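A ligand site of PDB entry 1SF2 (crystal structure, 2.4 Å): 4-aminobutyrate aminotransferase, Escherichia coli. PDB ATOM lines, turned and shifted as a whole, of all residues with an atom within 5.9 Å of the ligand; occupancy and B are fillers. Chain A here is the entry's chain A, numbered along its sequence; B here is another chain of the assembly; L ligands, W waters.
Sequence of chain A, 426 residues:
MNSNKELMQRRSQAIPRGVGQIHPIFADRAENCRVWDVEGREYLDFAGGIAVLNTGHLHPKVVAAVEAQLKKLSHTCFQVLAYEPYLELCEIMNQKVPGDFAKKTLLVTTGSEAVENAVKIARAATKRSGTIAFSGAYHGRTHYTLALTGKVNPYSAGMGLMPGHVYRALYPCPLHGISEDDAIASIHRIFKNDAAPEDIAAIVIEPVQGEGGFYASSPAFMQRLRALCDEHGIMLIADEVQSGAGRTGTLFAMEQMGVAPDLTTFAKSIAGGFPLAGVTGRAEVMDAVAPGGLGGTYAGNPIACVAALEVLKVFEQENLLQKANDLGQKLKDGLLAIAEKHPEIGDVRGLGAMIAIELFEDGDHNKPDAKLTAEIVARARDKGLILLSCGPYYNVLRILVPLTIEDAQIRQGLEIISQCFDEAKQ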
ATOM      1  N   ILE A  50       4.920  10.854 -14.876  1.00  0.00           N
ATOM      2  CA  ILE A  50       5.624   9.922 -15.744  1.00  0.00           C
ATOM      3  C   ILE A  50       5.023   8.527 -15.647  1.00  0.00           C
ATOM      4  O   ILE A  50       5.672   7.591 -15.166  1.00  0.00           O
ATOM      5  CB  ILE A  50       7.140   9.799 -15.478  1.00  0.00           C
ATOM      6  CG1 ILE A  50       7.798  11.178 -15.352  1.00  0.00           C
ATOM      7  CG2 ILE A  50       7.807   9.091 -16.670  1.00  0.00           C
ATOM      8  CD1 ILE A  50       9.329  11.130 -15.380  1.00  0.00           C
ATOM      9  N   THR A 109      11.232  -1.329  -3.916  1.00  0.00           N
ATOM     10  CA  THR A 109      10.673   0.016  -3.799  1.00  0.00           C
ATOM     11  C   THR A 109      10.617   0.825  -5.099  1.00  0.00           C
ATOM     12  O   THR A 109       9.603   1.480  -5.363  1.00  0.00           O
ATOM     13  CB  THR A 109      11.446   0.793  -2.686  1.00  0.00           C
ATOM     14  OG1 THR A 109      11.332   0.062  -1.444  1.00  0.00           O
ATOM     15  CG2 THR A 109      10.860   2.212  -2.484  1.00  0.00           C
ATOM     16  N   THR A 110      11.678   0.782  -5.904  1.00  0.00           N
ATOM     17  CA  THR A 110      11.702   1.528  -7.169  1.00  0.00           C
ATOM     18  C   THR A 110      11.864   0.610  -8.402  1.00  0.00           C
ATOM     19  O   THR A 110      12.297  -0.541  -8.282  1.00  0.00           O
ATOM     20  CB  THR A 110      12.866   2.576  -7.194  1.00  0.00           C
ATOM     21  OG1 THR A 110      14.112   1.895  -7.371  1.00  0.00           O
ATOM     22  CG2 THR A 110      12.905   3.378  -5.872  1.00  0.00           C
ATOM     23  N   GLY A 111      11.516   1.123  -9.582  1.00  0.00           N
ATOM     24  CA  GLY A 111      11.648   0.360 -10.819  1.00  0.00           C
ATOM     25  C   GLY A 111      13.092  -0.058 -11.036  1.00  0.00           C
ATOM     26  O   GLY A 111      13.359  -1.188 -11.482  1.00  0.00           O
ATOM     27  N   SER A 112      14.024   0.844 -10.733  1.00  0.00           N
ATOM     28  CA  SER A 112      15.441   0.531 -10.895  1.00  0.00           C
ATOM     29  C   SER A 112      15.788  -0.697 -10.060  1.00  0.00           C
ATOM     30  O   SER A 112      16.429  -1.625 -10.551  1.00  0.00           O
ATOM     31  CB  SER A 112      16.308   1.708 -10.444  1.00  0.00           C
ATOM     32  OG  SER A 112      16.112   2.829 -11.289  1.00  0.00           O
ATOM     33  N   GLU A 113      15.365  -0.702  -8.796  1.00  0.00           N
ATOM     34  CA  GLU A 113      15.651  -1.827  -7.906  1.00  0.00           C
ATOM     35  C   GLU A 113      14.993  -3.081  -8.488  1.00  0.00           C
ATOM     36  O   GLU A 113      15.554  -4.168  -8.437  1.00  0.00           O
ATOM     37  CB  GLU A 113      15.083  -1.596  -6.502  1.00  0.00           C
ATOM     38  CG  GLU A 113      15.748  -0.520  -5.699  1.00  0.00           C
ATOM     39  CD  GLU A 113      15.289  -0.558  -4.247  1.00  0.00           C
ATOM     40  OE1 GLU A 113      14.078  -0.770  -4.004  1.00  0.00           O
ATOM     41  OE2 GLU A 113      16.145  -0.367  -3.342  1.00  0.00           O
ATOM     42  N   VAL A 115      14.423  -3.848 -11.645  1.00  0.00           N
ATOM     43  CA  VAL A 115      15.217  -4.379 -12.744  1.00  0.00           C
ATOM     44  C   VAL A 115      16.502  -4.985 -12.196  1.00  0.00           C
ATOM     45  O   VAL A 115      16.953  -6.014 -12.674  1.00  0.00           O
ATOM     46  CB  VAL A 115      15.566  -3.290 -13.802  1.00  0.00           C
ATOM     47  CG1 VAL A 115      16.494  -3.891 -14.862  1.00  0.00           C
ATOM     48  CG2 VAL A 115      14.277  -2.761 -14.457  1.00  0.00           C
ATOM     49  N   TYR A 138      15.329   2.018 -21.522  1.00  0.00           N
ATOM     50  CA  TYR A 138      15.491   2.770 -20.282  1.00  0.00           C
ATOM     51  C   TYR A 138      15.150   1.829 -19.136  1.00  0.00           C
ATOM     52  O   TYR A 138      14.029   1.290 -19.082  1.00  0.00           O
ATOM     53  CB  TYR A 138      14.579   3.985 -20.218  1.00  0.00           C
ATOM     54  CG  TYR A 138      14.860   4.755 -18.963  1.00  0.00           C
ATOM     55  CD1 TYR A 138      15.973   5.594 -18.886  1.00  0.00           C
ATOM     56  CD2 TYR A 138      14.059   4.613 -17.827  1.00  0.00           C
ATOM     57  CE1 TYR A 138      16.284   6.268 -17.717  1.00  0.00           C
ATOM     58  CE2 TYR A 138      14.373   5.277 -16.639  1.00  0.00           C
ATOM     59  CZ  TYR A 138      15.483   6.104 -16.593  1.00  0.00           C
ATOM     60  OH  TYR A 138      15.785   6.811 -15.452  1.00  0.00           O
ATOM     61  N   HIS A 139      16.079   1.625 -18.208  1.00  0.00           N
ATOM     62  CA  HIS A 139      15.838   0.693 -17.135  1.00  0.00           C
ATOM     63  C   HIS A 139      16.149   1.222 -15.731  1.00  0.00           C
ATOM     64  O   HIS A 139      16.024   0.482 -14.748  1.00  0.00           O
ATOM     65  CB  HIS A 139      16.632  -0.591 -17.396  1.00  0.00           C
ATOM     66  CG  HIS A 139      16.258  -1.273 -18.681  1.00  0.00           C
ATOM     67  ND1 HIS A 139      15.025  -1.865 -18.888  1.00  0.00           N
ATOM     68  CD2 HIS A 139      16.979  -1.514 -19.808  1.00  0.00           C
ATOM     69  CE1 HIS A 139      15.010  -2.438 -20.082  1.00  0.00           C
ATOM     70  NE2 HIS A 139      16.178  -2.230 -20.658  1.00  0.00           N
ATOM     71  N   GLY A 140      16.542   2.478 -15.632  1.00  0.00           N
ATOM     72  CA  GLY A 140      16.871   3.019 -14.317  1.00  0.00           C
ATOM     73  C   GLY A 140      18.215   3.737 -14.255  1.00  0.00           C
ATOM     74  O   GLY A 140      19.036   3.675 -15.175  1.00  0.00           O
ATOM     75  N   ARG A 141      18.441   4.372 -13.114  1.00  0.00           N
ATOM     76  CA  ARG A 141      19.629   5.175 -12.905  1.00  0.00           C
ATOM     77  C   ARG A 141      20.681   4.646 -11.935  1.00  0.00           C
ATOM     78  O   ARG A 141      21.500   5.422 -11.455  1.00  0.00           O
ATOM     79  CB  ARG A 141      19.213   6.586 -12.474  1.00  0.00           C
ATOM     80  CG  ARG A 141      18.520   7.381 -13.565  1.00  0.00           C
ATOM     81  CD  ARG A 141      17.778   8.583 -12.968  1.00  0.00           C
ATOM     82  NE  ARG A 141      17.149   9.435 -13.983  1.00  0.00           N
ATOM     83  CZ  ARG A 141      17.782  10.332 -14.729  1.00  0.00           C
ATOM     84  NH1 ARG A 141      19.087  10.545 -14.582  1.00  0.00           N
ATOM     85  NH2 ARG A 141      17.096  11.041 -15.617  1.00  0.00           N
ATOM     86  N   GLU A 206      11.624  -3.872 -23.060  1.00  0.00           N
ATOM     87  CA  GLU A 206      10.389  -3.186 -22.719  1.00  0.00           C
ATOM     88  C   GLU A 206       9.383  -3.613 -23.797  1.00  0.00           C
ATOM     89  O   GLU A 206       9.637  -3.378 -24.988  1.00  0.00           O
ATOM     90  CB  GLU A 206      10.577  -1.670 -22.786  1.00  0.00           C
ATOM     91  CG  GLU A 206      11.285  -1.057 -21.587  1.00  0.00           C
ATOM     92  CD  GLU A 206      11.944   0.257 -21.935  1.00  0.00           C
ATOM     93  OE1 GLU A 206      13.043   0.214 -22.521  1.00  0.00           O
ATOM     94  OE2 GLU A 206      11.369   1.323 -21.637  1.00  0.00           O
ATOM     95  N   GLY A 210       9.454   3.090 -23.291  1.00  0.00           N
ATOM     96  CA  GLY A 210       8.904   4.318 -22.732  1.00  0.00           C
ATOM     97  C   GLY A 210       9.680   5.545 -23.110  1.00  0.00           C
ATOM     98  O   GLY A 210       9.283   6.284 -24.013  1.00  0.00           O
ATOM     99  N   GLU A 211      10.796   5.776 -22.421  1.00  0.00           N
ATOM    100  CA  GLU A 211      11.663   6.930 -22.684  1.00  0.00           C
ATOM    101  C   GLU A 211      12.248   6.768 -24.069  1.00  0.00           C
ATOM    102  O   GLU A 211      12.619   7.745 -24.719  1.00  0.00           O
ATOM    103  CB  GLU A 211      12.785   6.988 -21.648  1.00  0.00           C
ATOM    104  CG  GLU A 211      12.299   6.937 -20.198  1.00  0.00           C
ATOM    105  CD  GLU A 211      11.324   8.058 -19.867  1.00  0.00           C
ATOM    106  OE1 GLU A 211      11.702   9.234 -20.008  1.00  0.00           O
ATOM    107  OE2 GLU A 211      10.180   7.773 -19.449  1.00  0.00           O
ATOM    108  N   ASP A 239      10.556  -5.670 -18.935  1.00  0.00           N
ATOM    109  CA  ASP A 239      10.534  -4.518 -18.061  1.00  0.00           C
ATOM    110  C   ASP A 239       9.229  -3.768 -18.335  1.00  0.00           C
ATOM    111  O   ASP A 239       9.110  -3.052 -19.337  1.00  0.00           O
ATOM    112  CB  ASP A 239      11.725  -3.593 -18.330  1.00  0.00           C
ATOM    113  CG  ASP A 239      11.795  -2.431 -17.349  1.00  0.00           C
ATOM    114  OD1 ASP A 239      10.809  -2.235 -16.592  1.00  0.00           O
ATOM    115  OD2 ASP A 239      12.823  -1.706 -17.324  1.00  0.00           O
ATOM    116  N   GLU A 240       8.263  -3.946 -17.433  1.00  0.00           N
ATOM    117  CA  GLU A 240       6.960  -3.305 -17.565  1.00  0.00           C
ATOM    118  C   GLU A 240       6.697  -2.211 -16.535  1.00  0.00           C
ATOM    119  O   GLU A 240       5.551  -1.916 -16.196  1.00  0.00           O
ATOM    120  CB  GLU A 240       5.858  -4.359 -17.508  1.00  0.00           C
ATOM    121  CG  GLU A 240       5.968  -5.372 -18.644  1.00  0.00           C
ATOM    122  CD  GLU A 240       4.656  -5.571 -19.396  1.00  0.00           C
ATOM    123  OE1 GLU A 240       3.969  -4.573 -19.684  1.00  0.00           O
ATOM    124  OE2 GLU A 240       4.317  -6.738 -19.718  1.00  0.00           O
ATOM    125  N   VAL A 241       7.777  -1.593 -16.048  1.00  0.00           N
ATOM    126  CA  VAL A 241       7.645  -0.509 -15.080  1.00  0.00           C
ATOM    127  C   VAL A 241       6.754   0.608 -15.635  1.00  0.00           C
ATOM    128  O   VAL A 241       5.989   1.219 -14.888  1.00  0.00           O
ATOM    129  CB  VAL A 241       9.018   0.081 -14.708  1.00  0.00           C
ATOM    130  CG1 VAL A 241       8.839   1.416 -14.018  1.00  0.00           C
ATOM    131  CG2 VAL A 241       9.771  -0.886 -13.810  1.00  0.00           C
ATOM    132  N   GLN A 242       6.862   0.880 -16.936  1.00  0.00           N
ATOM    133  CA  GLN A 242       6.057   1.938 -17.541  1.00  0.00           C
ATOM    134  C   GLN A 242       4.932   1.409 -18.419  1.00  0.00           C
ATOM    135  O   GLN A 242       3.859   1.988 -18.457  1.00  0.00           O
ATOM    136  CB  GLN A 242       6.945   2.904 -18.343  1.00  0.00           C
ATOM    137  CG  GLN A 242       6.185   4.095 -18.967  1.00  0.00           C
ATOM    138  CD  GLN A 242       7.099   5.235 -19.445  1.00  0.00           C
ATOM    139  OE1 GLN A 242       6.687   6.077 -20.255  1.00  0.00           O
ATOM    140  NE2 GLN A 242       8.341   5.264 -18.951  1.00  0.00           N
ATOM    141  N   SER A 243       5.172   0.317 -19.117  1.00  0.00           N
ATOM    142  CA  SER A 243       4.138  -0.239 -19.992  1.00  0.00           C
ATOM    143  C   SER A 243       3.078  -0.967 -19.168  1.00  0.00           C
ATOM    144  O   SER A 243       1.963  -1.156 -19.625  1.00  0.00           O
ATOM    145  CB  SER A 243       4.741  -1.211 -20.998  1.00  0.00           C
ATOM    146  OG  SER A 243       5.281  -2.325 -20.312  1.00  0.00           O
ATOM    147  N   ALA A 267       6.214  -1.196 -11.497  1.00  0.00           N
ATOM    148  CA  ALA A 267       6.364  -0.051 -10.593  1.00  0.00           C
ATOM    149  C   ALA A 267       5.457   1.075 -11.069  1.00  0.00           C
ATOM    150  O   ALA A 267       4.377   0.820 -11.592  1.00  0.00           O
ATOM    151  CB  ALA A 267       7.833   0.421 -10.591  1.00  0.00           C
ATOM    152  N   LYS A 268       5.886   2.314 -10.877  1.00  0.00           N
ATOM    153  CA  LYS A 268       5.119   3.486 -11.269  1.00  0.00           C
ATOM    154  C   LYS A 268       3.615   3.394 -10.961  1.00  0.00           C
ATOM    155  O   LYS A 268       3.223   3.490  -9.797  1.00  0.00           O
ATOM    156  CB  LYS A 268       5.346   3.777 -12.764  1.00  0.00           C
ATOM    157  CG  LYS A 268       6.782   4.180 -13.101  1.00  0.00           C
ATOM    158  CD  LYS A 268       6.905   4.755 -14.509  1.00  0.00           C
ATOM    159  CE  LYS A 268       8.254   5.458 -14.753  1.00  0.00           C
ATOM    160  NZ  LYS A 268       9.306   4.545 -15.277  1.00  0.00           N
ATOM    161  N   GLU B 113      19.977   3.494  -3.388  1.00  0.00           N
ATOM    162  CA  GLU B 113      19.989   4.558  -4.384  1.00  0.00           C
ATOM    163  C   GLU B 113      20.914   5.675  -3.964  1.00  0.00           C
ATOM    164  O   GLU B 113      21.665   6.201  -4.773  1.00  0.00           O
ATOM    165  CB  GLU B 113      18.585   5.110  -4.603  1.00  0.00           C
ATOM    166  CG  GLU B 113      17.669   4.171  -5.364  1.00  0.00           C
ATOM    167  CD  GLU B 113      16.370   4.818  -5.791  1.00  0.00           C
ATOM    168  OE1 GLU B 113      15.729   5.533  -4.963  1.00  0.00           O
ATOM    169  OE2 GLU B 113      15.981   4.605  -6.957  1.00  0.00           O
ATOM    170  N   GLY B 295      18.028  11.456 -11.287  1.00  0.00           N
ATOM    171  CA  GLY B 295      16.583  11.311 -11.283  1.00  0.00           C
ATOM    172  C   GLY B 295      16.055  10.114 -10.509  1.00  0.00           C
ATOM    173  O   GLY B 295      16.759   9.523  -9.674  1.00  0.00           O
ATOM    174  N   GLY B 296      14.811   9.762 -10.807  1.00  0.00           N
ATOM    175  CA  GLY B 296      14.169   8.666 -10.139  1.00  0.00           C
ATOM    176  C   GLY B 296      12.706   9.010 -10.046  1.00  0.00           C
ATOM    177  O   GLY B 296      12.341  10.096  -9.592  1.00  0.00           O
ATOM    178  N   THR B 297      11.859   8.108 -10.491  1.00  0.00           N
ATOM    179  CA  THR B 297      10.429   8.346 -10.465  1.00  0.00           C
ATOM    180  C   THR B 297       9.907   8.811  -9.107  1.00  0.00           C
ATOM    181  O   THR B 297       9.410   9.930  -8.988  1.00  0.00           O
ATOM    182  CB  THR B 297       9.673   7.096 -10.880  1.00  0.00           C
ATOM    183  OG1 THR B 297      10.112   6.699 -12.187  1.00  0.00           O
ATOM    184  CG2 THR B 297       8.189   7.367 -10.918  1.00  0.00           C
ATOM    185  N   TYR B 298      10.044   7.965  -8.096  1.00  0.00           N
ATOM    186  CA  TYR B 298       9.543   8.268  -6.753  1.00  0.00           C
ATOM    187  C   TYR B 298      10.432   9.186  -5.921  1.00  0.00           C
ATOM    188  O   TYR B 298      10.052   9.567  -4.822  1.00  0.00           O
ATOM    189  CB  TYR B 298       9.355   6.974  -5.952  1.00  0.00           C
ATOM    190  CG  TYR B 298       8.428   5.962  -6.576  1.00  0.00           C
ATOM    191  CD1 TYR B 298       7.169   6.324  -7.049  1.00  0.00           C
ATOM    192  CD2 TYR B 298       8.776   4.620  -6.606  1.00  0.00           C
ATOM    193  CE1 TYR B 298       6.288   5.367  -7.549  1.00  0.00           C
ATOM    194  CE2 TYR B 298       7.922   3.666  -7.093  1.00  0.00           C
ATOM    195  CZ  TYR B 298       6.678   4.035  -7.560  1.00  0.00           C
ATOM    196  OH  TYR B 298       5.807   3.058  -7.979  1.00  0.00           O
HETATM  197  N1  LIG L   1      12.351   0.884 -16.353  1.00  0.00           N
HETATM  198  C1  LIG L   1      11.413   1.544 -17.164  1.00  0.00           C
HETATM  199  C2  LIG L   1      10.846   0.840 -18.317  1.00  0.00           C
HETATM  200  C3  LIG L   1      10.940   2.837 -16.731  1.00  0.00           C
HETATM  201  O1  LIG L   1      10.248   3.672 -17.622  1.00  0.00           O
HETATM  202  C4  LIG L   1      11.379   3.350 -15.525  1.00  0.00           C
HETATM  203  C5  LIG L   1      10.623   4.566 -15.153  1.00  0.00           C
HETATM  204  C6  LIG L   1      12.282   2.650 -14.683  1.00  0.00           C
HETATM  205  C7  LIG L   1      12.763   1.386 -15.118  1.00  0.00           C
HETATM  206  C8  LIG L   1      12.987   3.048 -13.429  1.00  0.00           C
HETATM  207  O2  LIG L   1      11.996   3.257 -12.429  1.00  0.00           O
HETATM  208  P1  LIG L   1      12.280   4.166 -11.294  1.00  0.00           P
HETATM  209  O3  LIG L   1      11.093   4.141 -10.275  1.00  0.00           O
HETATM  210  O4  LIG L   1      12.413   5.679 -11.764  1.00  0.00           O
HETATM  211  O5  LIG L   1      13.653   3.764 -10.534  1.00  0.00           O
HETATM  212  O   HOH W   1      11.227   3.693 -20.422  1.00  0.00           O
HETATM  213  O   HOH W   2       7.936  -0.533 -19.313  1.00  0.00           O
HETATM  214  O   HOH W   3      11.499   5.558  -8.234  1.00  0.00           O
HETATM  215  O   HOH W   4       8.413   3.890 -10.372  1.00  0.00           O
HETATM  216  O   HOH W   5      10.158   7.295 -16.915  1.00  0.00           O
HETATM  217  O   HOH W   6      14.159   5.530  -8.646  1.00  0.00           O
HETATM  218  O   HOH W   7      16.049   5.447 -11.409  1.00  0.00           O
HETATM  219  O   HOH W   8      14.516   6.428 -13.237  1.00  0.00           O
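A carbon (C5) of the ligand is covalently linked to the side-chain amino group (NZ) of Lys 268. The backbone NH of Thr 297 of chain B is in hydrogen-bond range of an oxygen (O4) of the ligand. The side-chain hydroxyl of Thr 297 of chain B sits at hydrogen-bond distance from an oxygen (O4) of the ligand (2.6 Å). The backbone NH (N) of Ser 112 lies within hydrogen-bond range of an oxygen (O5) of the ligand (3.0 Å). OG of Ser 112 sits at hydrogen-bond distance from O5 of the ligand (2.7 Å). The side-chain carboxylate of Asp 239 lies within hydrogen-bond range of a nitrogen (N1) of the ligand (2.8 Å). NE2 of Gln 242 sits at hydrogen-bond distance from O1 of the ligand (2.8 Å). An oxygen (O3) of the ligand sits at hydrogen-bond distance from the backbone NH (N) of Gly 111 (3.1 Å).
The side-chain carboxylate (OD2) of Asp 239 lies within hydrogen-bond range of a ring nitrogen (ND1) of His 139 (2.7 Å). The backbone NH (N) of Val 241 lies within hydrogen-bond range of the side-chain carboxylate (OD1) of Asp 239, at 3.1 Å. The side-chain carboxylate of Glu 211 sits at hydrogen-bond distance from the side-chain amide nitrogen of Gln 242, at 3.2 Å. The side-chain carboxylate (OE1) of Glu 206 sits at hydrogen-bond distance from the backbone NH (N) of Tyr 138 (3.1 Å). The guanidinium group (NE) of Arg 141 sits at hydrogen-bond distance from the side-chain hydroxyl (OH) of Tyr 138, 3.3 Å away. OE2 of Glu 206 lies within hydrogen-bond range of N of Gly 210 (3.1 Å). OG1 of Thr 110 lies within hydrogen-bond range of OE2 of Glu 113 of chain B (3.3 Å). N of Glu 113 of chain A is in hydrogen-bond range of OG1 of Thr 110, at 3.2 Å.
O of Tyr 138 lies close to N1 of the ligand (3.2 Å). CB of Thr 110 touches O5 of the ligand (3.6 Å). His 139 touches the ligand. Gly 140 touches the ligand. Glu 206 touches the ligand. Val 241 touches the ligand. Gly 296 of chain B touches the ligand. Of the 26 residues printed, 13 come within 4 Å of the ligand. Along chain A the residues within 4 Å of the ligand span positions 110 to 268. The nearest printed residue that does not touch the ligand is Glu 113 of chain B (4.3 Å).
Water W3 lies within hydrogen-bond range of O3 of the ligand (2.5 Å), N of Tyr 298 of chain B (2.8 Å) and N of Thr 297 of chain B (3.4 Å). Water W6 lies within hydrogen-bond range of an oxygen (O5) of the ligand (2.6 Å) and the side-chain carboxylate of Glu 113 of chain B (2.7 Å). Water W8 bridges the side-chain hydroxyl of Tyr 138 and an oxygen (O4) of the ligand. Water W4 bridges O3 of the ligand (2.7 Å) and N of Lys 268 (3.0 Å). Water W1 lies within hydrogen-bond range of the side-chain carboxylate (OE2) of Glu 206 (2.7 Å), the backbone NH (N) of Glu 211 (2.9 Å), an oxygen (O1) of the ligand (3.0 Å) and the backbone NH (N) of Gly 210 (3.4 Å). Water W5 lies within hydrogen-bond range of OE2 of Glu 211 (2.6 Å), NZ of Lys 268 (3.3 Å) and NE2 of Gln 242 (3.4 Å).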
